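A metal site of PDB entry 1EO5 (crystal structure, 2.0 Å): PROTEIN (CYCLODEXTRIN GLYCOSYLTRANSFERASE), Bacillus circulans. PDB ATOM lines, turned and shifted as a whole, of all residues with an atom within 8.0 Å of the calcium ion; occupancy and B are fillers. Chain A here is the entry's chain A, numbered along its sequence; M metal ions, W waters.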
ATOM      1  N   PRO A 138     -27.368  19.420   5.029  1.00  0.00           N
ATOM      2  CA  PRO A 138     -26.600  19.444   6.276  1.00  0.00           C
ATOM      3  C   PRO A 138     -25.374  20.358   6.221  1.00  0.00           C
ATOM      4  O   PRO A 138     -24.565  20.363   7.151  1.00  0.00           O
ATOM      5  CB  PRO A 138     -26.163  17.994   6.435  1.00  0.00           C
ATOM      6  CG  PRO A 138     -26.066  17.477   5.047  1.00  0.00           C
ATOM      7  CD  PRO A 138     -27.153  18.172   4.273  1.00  0.00           C
ATOM      8  N   ASN A 139     -25.253  21.157   5.162  1.00  0.00           N
ATOM      9  CA  ASN A 139     -24.117  22.068   5.050  1.00  0.00           C
ATOM     10  C   ASN A 139     -24.250  23.263   5.976  1.00  0.00           C
ATOM     11  O   ASN A 139     -23.251  23.834   6.407  1.00  0.00           O
ATOM     12  CB  ASN A 139     -23.972  22.576   3.614  1.00  0.00           C
ATOM     13  CG  ASN A 139     -22.876  23.629   3.483  1.00  0.00           C
ATOM     14  OD1 ASN A 139     -21.689  23.328   3.600  1.00  0.00           O
ATOM     15  ND2 ASN A 139     -23.269  24.869   3.226  1.00  0.00           N
ATOM     16  N   HIS A 140     -25.480  23.683   6.227  1.00  0.00           N
ATOM     17  CA  HIS A 140     -25.705  24.904   6.972  1.00  0.00           C
ATOM     18  C   HIS A 140     -27.069  24.934   7.626  1.00  0.00           C
ATOM     19  O   HIS A 140     -27.923  24.089   7.350  1.00  0.00           O
ATOM     20  CB  HIS A 140     -25.637  26.075   6.012  1.00  0.00           C
ATOM     21  CG  HIS A 140     -26.537  25.906   4.822  1.00  0.00           C
ATOM     22  ND1 HIS A 140     -26.083  25.441   3.604  1.00  0.00           N
ATOM     23  CD2 HIS A 140     -27.879  25.998   4.703  1.00  0.00           C
ATOM     24  CE1 HIS A 140     -27.092  25.319   2.771  1.00  0.00           C
ATOM     25  NE2 HIS A 140     -28.199  25.663   3.415  1.00  0.00           N
ATOM     26  N   HIS A 176     -18.683  27.464  11.252  1.00  0.00           N
ATOM     27  CA  HIS A 176     -17.411  28.039  10.829  1.00  0.00           C
ATOM     28  C   HIS A 176     -17.508  29.542  10.896  1.00  0.00           C
ATOM     29  O   HIS A 176     -18.558  30.119  10.639  1.00  0.00           O
ATOM     30  CB  HIS A 176     -17.085  27.621   9.396  1.00  0.00           C
ATOM     31  CG  HIS A 176     -16.652  26.194   9.263  1.00  0.00           C
ATOM     32  ND1 HIS A 176     -17.168  25.349   8.307  1.00  0.00           N
ATOM     33  CD2 HIS A 176     -15.761  25.472   9.971  1.00  0.00           C
ATOM     34  CE1 HIS A 176     -16.603  24.156   8.430  1.00  0.00           C
ATOM     35  NE2 HIS A 176     -15.749  24.206   9.443  1.00  0.00           N
ATOM     36  N   GLU A 187     -11.350  24.090  -1.236  1.00  0.00           N
ATOM     37  CA  GLU A 187     -11.182  24.285   0.195  1.00  0.00           C
ATOM     38  C   GLU A 187     -11.912  25.542   0.647  1.00  0.00           C
ATOM     39  O   GLU A 187     -12.631  25.532   1.645  1.00  0.00           O
ATOM     40  CB  GLU A 187      -9.687  24.398   0.558  1.00  0.00           C
ATOM     41  CG  GLU A 187      -9.422  24.773   2.006  1.00  0.00           C
ATOM     42  CD  GLU A 187      -7.975  25.162   2.256  1.00  0.00           C
ATOM     43  OE1 GLU A 187      -7.237  25.380   1.273  1.00  0.00           O
ATOM     44  OE2 GLU A 187      -7.562  25.245   3.434  1.00  0.00           O
ATOM     45  N   ASN A 188     -11.733  26.618  -0.115  1.00  0.00           N
ATOM     46  CA  ASN A 188     -12.382  27.886   0.184  1.00  0.00           C
ATOM     47  C   ASN A 188     -13.901  27.722   0.237  1.00  0.00           C
ATOM     48  O   ASN A 188     -14.559  28.260   1.128  1.00  0.00           O
ATOM     49  CB  ASN A 188     -12.000  28.924  -0.872  1.00  0.00           C
ATOM     50  CG  ASN A 188     -12.511  30.306  -0.536  1.00  0.00           C
ATOM     51  OD1 ASN A 188     -13.685  30.619  -0.737  1.00  0.00           O
ATOM     52  ND2 ASN A 188     -11.613  31.162  -0.059  1.00  0.00           N
ATOM     53  N   GLY A 189     -14.439  26.985  -0.714  1.00  0.00           N
ATOM     54  CA  GLY A 189     -15.882  26.776  -0.812  1.00  0.00           C
ATOM     55  C   GLY A 189     -16.408  25.843   0.273  1.00  0.00           C
ATOM     56  O   GLY A 189     -17.609  25.834   0.564  1.00  0.00           O
ATOM     57  N   ILE A 190     -15.527  25.049   0.860  1.00  0.00           N
ATOM     58  CA  ILE A 190     -15.944  24.099   1.888  1.00  0.00           C
ATOM     59  C   ILE A 190     -15.939  24.706   3.278  1.00  0.00           C
ATOM     60  O   ILE A 190     -16.882  24.532   4.043  1.00  0.00           O
ATOM     61  CB  ILE A 190     -15.056  22.834   1.892  1.00  0.00           C
ATOM     62  CG1 ILE A 190     -15.314  21.989   0.649  1.00  0.00           C
ATOM     63  CG2 ILE A 190     -15.301  22.018   3.152  1.00  0.00           C
ATOM     64  CD1 ILE A 190     -14.377  20.810   0.501  1.00  0.00           C
ATOM     65  N   TYR A 191     -14.858  25.387   3.621  1.00  0.00           N
ATOM     66  CA  TYR A 191     -14.686  25.898   4.976  1.00  0.00           C
ATOM     67  C   TYR A 191     -15.109  27.344   5.208  1.00  0.00           C
ATOM     68  O   TYR A 191     -14.900  27.897   6.290  1.00  0.00           O
ATOM     69  CB  TYR A 191     -13.280  25.628   5.489  1.00  0.00           C
ATOM     70  CG  TYR A 191     -12.973  24.152   5.543  1.00  0.00           C
ATOM     71  CD1 TYR A 191     -13.445  23.372   6.591  1.00  0.00           C
ATOM     72  CD2 TYR A 191     -12.368  23.513   4.476  1.00  0.00           C
ATOM     73  CE1 TYR A 191     -13.230  22.007   6.624  1.00  0.00           C
ATOM     74  CE2 TYR A 191     -12.148  22.145   4.493  1.00  0.00           C
ATOM     75  CZ  TYR A 191     -12.583  21.393   5.569  1.00  0.00           C
ATOM     76  OH  TYR A 191     -12.368  20.035   5.594  1.00  0.00           O
ATOM     77  N   LYS A 192     -15.778  27.929   4.224  1.00  0.00           N
ATOM     78  CA  LYS A 192     -16.331  29.270   4.359  1.00  0.00           C
ATOM     79  C   LYS A 192     -17.825  29.199   4.076  1.00  0.00           C
ATOM     80  O   LYS A 192     -18.299  28.218   3.512  1.00  0.00           O
ATOM     81  CB  LYS A 192     -15.648  30.235   3.386  1.00  0.00           C
ATOM     82  CG  LYS A 192     -14.142  30.292   3.520  1.00  0.00           C
ATOM     83  CD  LYS A 192     -13.573  31.563   2.896  1.00  0.00           C
ATOM     84  CE  LYS A 192     -12.246  31.938   3.527  1.00  0.00           C
ATOM     85  NZ  LYS A 192     -11.631  33.119   2.848  1.00  0.00           N
ATOM     86  N   ASN A 193     -18.557  30.219   4.486  1.00  0.00           N
ATOM     87  CA  ASN A 193     -20.012  30.233   4.309  1.00  0.00           C
ATOM     88  C   ASN A 193     -20.446  30.326   2.858  1.00  0.00           C
ATOM     89  O   ASN A 193     -19.842  31.040   2.061  1.00  0.00           O
ATOM     90  CB  ASN A 193     -20.644  31.399   5.073  1.00  0.00           C
ATOM     91  CG  ASN A 193     -20.453  31.291   6.551  1.00  0.00           C
ATOM     92  OD1 ASN A 193     -20.221  30.208   7.089  1.00  0.00           O
ATOM     93  ND2 ASN A 193     -20.556  32.424   7.243  1.00  0.00           N
ATOM     94  N   LEU A 194     -21.570  29.681   2.563  1.00  0.00           N
ATOM     95  CA  LEU A 194     -22.229  29.816   1.272  1.00  0.00           C
ATOM     96  C   LEU A 194     -23.143  31.026   1.436  1.00  0.00           C
ATOM     97  O   LEU A 194     -24.080  30.986   2.243  1.00  0.00           O
ATOM     98  CB  LEU A 194     -23.082  28.576   1.013  1.00  0.00           C
ATOM     99  CG  LEU A 194     -22.694  27.609  -0.083  1.00  0.00           C
ATOM    100  CD1 LEU A 194     -23.947  27.137  -0.777  1.00  0.00           C
ATOM    101  CD2 LEU A 194     -21.744  28.268  -1.094  1.00  0.00           C
ATOM    102  N   LEU A 197     -25.119  32.056   4.808  1.00  0.00           N
ATOM    103  CA  LEU A 197     -25.596  30.894   5.546  1.00  0.00           C
ATOM    104  C   LEU A 197     -24.578  30.405   6.578  1.00  0.00           C
ATOM    105  O   LEU A 197     -23.402  30.229   6.266  1.00  0.00           O
ATOM    106  CB  LEU A 197     -25.959  29.753   4.589  1.00  0.00           C
ATOM    107  CG  LEU A 197     -26.934  30.106   3.459  1.00  0.00           C
ATOM    108  CD1 LEU A 197     -27.020  28.969   2.451  1.00  0.00           C
ATOM    109  CD2 LEU A 197     -28.313  30.434   4.020  1.00  0.00           C
ATOM    110  N   ALA A 198     -25.050  30.194   7.798  1.00  0.00           N
ATOM    111  CA  ALA A 198     -24.188  29.712   8.877  1.00  0.00           C
ATOM    112  C   ALA A 198     -23.646  28.330   8.541  1.00  0.00           C
ATOM    113  O   ALA A 198     -24.396  27.355   8.472  1.00  0.00           O
ATOM    114  CB  ALA A 198     -24.962  29.668  10.197  1.00  0.00           C
ATOM    115  N   ASP A 199     -22.338  28.256   8.296  1.00  0.00           N
ATOM    116  CA  ASP A 199     -21.708  27.001   7.913  1.00  0.00           C
ATOM    117  C   ASP A 199     -21.529  26.053   9.093  1.00  0.00           C
ATOM    118  O   ASP A 199     -20.836  26.377  10.058  1.00  0.00           O
ATOM    119  CB  ASP A 199     -20.362  27.244   7.226  1.00  0.00           C
ATOM    120  CG  ASP A 199     -20.048  26.198   6.179  1.00  0.00           C
ATOM    121  OD1 ASP A 199     -20.901  25.952   5.299  1.00  0.00           O
ATOM    122  OD2 ASP A 199     -18.944  25.614   6.239  1.00  0.00           O
ATOM    123  N   LEU A 200     -22.138  24.886   8.996  1.00  0.00           N
ATOM    124  CA  LEU A 200     -22.018  23.885  10.046  1.00  0.00           C
ATOM    125  C   LEU A 200     -20.611  23.315  10.063  1.00  0.00           C
ATOM    126  O   LEU A 200     -20.006  23.086   9.009  1.00  0.00           O
ATOM    127  CB  LEU A 200     -23.043  22.775   9.852  1.00  0.00           C
ATOM    128  CG  LEU A 200     -24.489  23.117  10.262  1.00  0.00           C
ATOM    129  CD1 LEU A 200     -25.457  22.058   9.776  1.00  0.00           C
ATOM    130  CD2 LEU A 200     -24.586  23.297  11.762  1.00  0.00           C
ATOM    131  N   ASN A 201     -20.080  23.111  11.263  1.00  0.00           N
ATOM    132  CA  ASN A 201     -18.747  22.557  11.432  1.00  0.00           C
ATOM    133  C   ASN A 201     -18.851  21.067  11.731  1.00  0.00           C
ATOM    134  O   ASN A 201     -19.106  20.676  12.867  1.00  0.00           O
ATOM    135  CB  ASN A 201     -18.027  23.274  12.570  1.00  0.00           C
ATOM    136  CG  ASN A 201     -16.695  22.650  12.892  1.00  0.00           C
ATOM    137  OD1 ASN A 201     -16.183  21.823  12.128  1.00  0.00           O
ATOM    138  ND2 ASN A 201     -16.113  23.037  14.024  1.00  0.00           N
ATOM    139  N   HIS A 202     -18.672  20.255  10.696  1.00  0.00           N
ATOM    140  CA  HIS A 202     -18.817  18.808  10.831  1.00  0.00           C
ATOM    141  C   HIS A 202     -17.679  18.151  11.599  1.00  0.00           C
ATOM    142  O   HIS A 202     -17.715  16.949  11.850  1.00  0.00           O
ATOM    143  CB  HIS A 202     -19.009  18.163   9.461  1.00  0.00           C
ATOM    144  CG  HIS A 202     -20.211  18.678   8.725  1.00  0.00           C
ATOM    145  ND1 HIS A 202     -20.131  19.686   7.777  1.00  0.00           N
ATOM    146  CD2 HIS A 202     -21.529  18.395   8.858  1.00  0.00           C
ATOM    147  CE1 HIS A 202     -21.338  19.953   7.330  1.00  0.00           C
ATOM    148  NE2 HIS A 202     -22.201  19.192   7.961  1.00  0.00           N
ATOM    149  N   ALA A 230     -25.530  21.168  -1.970  1.00  0.00           N
ATOM    150  CA  ALA A 230     -24.204  21.783  -1.852  1.00  0.00           C
ATOM    151  C   ALA A 230     -23.088  20.828  -1.427  1.00  0.00           C
ATOM    152  O   ALA A 230     -22.309  21.139  -0.529  1.00  0.00           O
ATOM    153  CB  ALA A 230     -24.266  22.983  -0.908  1.00  0.00           C
ATOM    154  N   VAL A 231     -22.981  19.695  -2.105  1.00  0.00           N
ATOM    155  CA  VAL A 231     -21.957  18.714  -1.759  1.00  0.00           C
ATOM    156  C   VAL A 231     -20.528  19.188  -2.002  1.00  0.00           C
ATOM    157  O   VAL A 231     -19.596  18.674  -1.401  1.00  0.00           O
ATOM    158  CB  VAL A 231     -22.199  17.350  -2.418  1.00  0.00           C
ATOM    159  CG1 VAL A 231     -23.513  16.741  -1.918  1.00  0.00           C
ATOM    160  CG2 VAL A 231     -22.209  17.489  -3.936  1.00  0.00           C
ATOM    161  N   LYS A 232     -20.354  20.178  -2.857  1.00  0.00           N
ATOM    162  CA  LYS A 232     -19.028  20.714  -3.111  1.00  0.00           C
ATOM    163  C   LYS A 232     -18.594  21.631  -1.966  1.00  0.00           C
ATOM    164  O   LYS A 232     -17.476  22.125  -1.946  1.00  0.00           O
ATOM    165  CB  LYS A 232     -18.961  21.462  -4.448  1.00  0.00           C
ATOM    166  CG  LYS A 232     -17.538  21.698  -4.952  1.00  0.00           C
ATOM    167  CD  LYS A 232     -17.509  22.496  -6.243  1.00  0.00           C
ATOM    168  CE  LYS A 232     -16.075  22.669  -6.763  1.00  0.00           C
ATOM    169  NZ  LYS A 232     -15.967  23.737  -7.792  1.00  0.00           N
ATOM    170  N   HIS A 233     -19.487  21.819  -0.989  1.00  0.00           N
ATOM    171  CA  HIS A 233     -19.215  22.731   0.110  1.00  0.00           C
ATOM    172  C   HIS A 233     -19.145  22.090   1.492  1.00  0.00           C
ATOM    173  O   HIS A 233     -19.120  22.774   2.504  1.00  0.00           O
ATOM    174  CB  HIS A 233     -20.180  23.890   0.091  1.00  0.00           C
ATOM    175  CG  HIS A 233     -20.212  24.606  -1.221  1.00  0.00           C
ATOM    176  ND1 HIS A 233     -19.335  25.615  -1.529  1.00  0.00           N
ATOM    177  CD2 HIS A 233     -20.877  24.321  -2.368  1.00  0.00           C
ATOM    178  CE1 HIS A 233     -19.530  25.998  -2.781  1.00  0.00           C
ATOM    179  NE2 HIS A 233     -20.448  25.231  -3.311  1.00  0.00           N
ATOM    180  N   MET A 234     -19.040  20.767   1.509  1.00  0.00           N
ATOM    181  CA  MET A 234     -18.857  20.020   2.738  1.00  0.00           C
ATOM    182  C   MET A 234     -17.633  19.130   2.557  1.00  0.00           C
ATOM    183  O   MET A 234     -17.320  18.724   1.433  1.00  0.00           O
ATOM    184  CB  MET A 234     -20.096  19.165   3.051  1.00  0.00           C
ATOM    185  CG  MET A 234     -21.361  19.983   3.317  1.00  0.00           C
ATOM    186  SD  MET A 234     -22.797  18.942   3.690  1.00  0.00           S
ATOM    187  CE  MET A 234     -23.257  18.390   2.052  1.00  0.00           C
ATOM    188  N   PRO A 235     -16.921  18.842   3.638  1.00  0.00           N
ATOM    189  CA  PRO A 235     -15.724  18.003   3.544  1.00  0.00           C
ATOM    190  C   PRO A 235     -16.091  16.667   2.910  1.00  0.00           C
ATOM    191  O   PRO A 235     -17.033  15.999   3.342  1.00  0.00           O
ATOM    192  CB  PRO A 235     -15.311  17.821   5.008  1.00  0.00           C
ATOM    193  CG  PRO A 235     -15.882  18.996   5.712  1.00  0.00           C
ATOM    194  CD  PRO A 235     -17.185  19.262   5.019  1.00  0.00           C
HETATM  195 CA    CA M   1     -19.490  24.096   4.403  1.00  0.00          CA
HETATM  196  O   HOH W   1     -19.378  25.864   2.755  1.00  0.00           O
HETATM  197  O   HOH W   2     -18.006  22.519   5.438  1.00  0.00           O
HETATM  198  O   HOH W   3     -20.635  23.193   6.373  1.00  0.00           O
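The backbone NH of Asp 199 sits close to the side-chain amide oxygen of Asn 193, at 3.1 Å.
The backbone carbonyl oxygen (O) of Asn 139 sits at hydrogen-bond distance from the backbone NH (N) of Leu 200 (3.0 Å).
The backbone NH (N) of Asn 139 sits at hydrogen-bond distance from the side-chain sulfur (SD) of Met 234 (3.6 Å).
A ring nitrogen (ND1) of His 233 is in hydrogen-bond range of the backbone carbonyl oxygen (O) of Gly 189, at 2.7 Å.
A ring nitrogen (ND1) of His 140 lies within hydrogen-bond range of the side-chain amide nitrogen (ND2) of Asn 139 (2.9 Å).
The backbone carbonyl oxygen (O) of Asp 199 is in hydrogen-bond range of the backbone NH (N) of His 176 (2.7 Å).
Along chain A the residues within 4 Å of the calcium ion span positions 139 to 233.
The calcium ion is bound by the backbone carbonyl oxygen (O) of His 233, water W2, water W1, the side-chain carboxylate (OD2) of Asp 199, water W3, the side-chain amide oxygen (OD1) of Asn 139, the side-chain carboxylate (OD1) of Asp 199 and the backbone carbonyl oxygen (O) of Ile 190.
Water W3 bridges the backbone carbonyl oxygen of Asn 139 (2.7 Å) and the backbone carbonyl oxygen of Leu 200 (2.7 Å).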
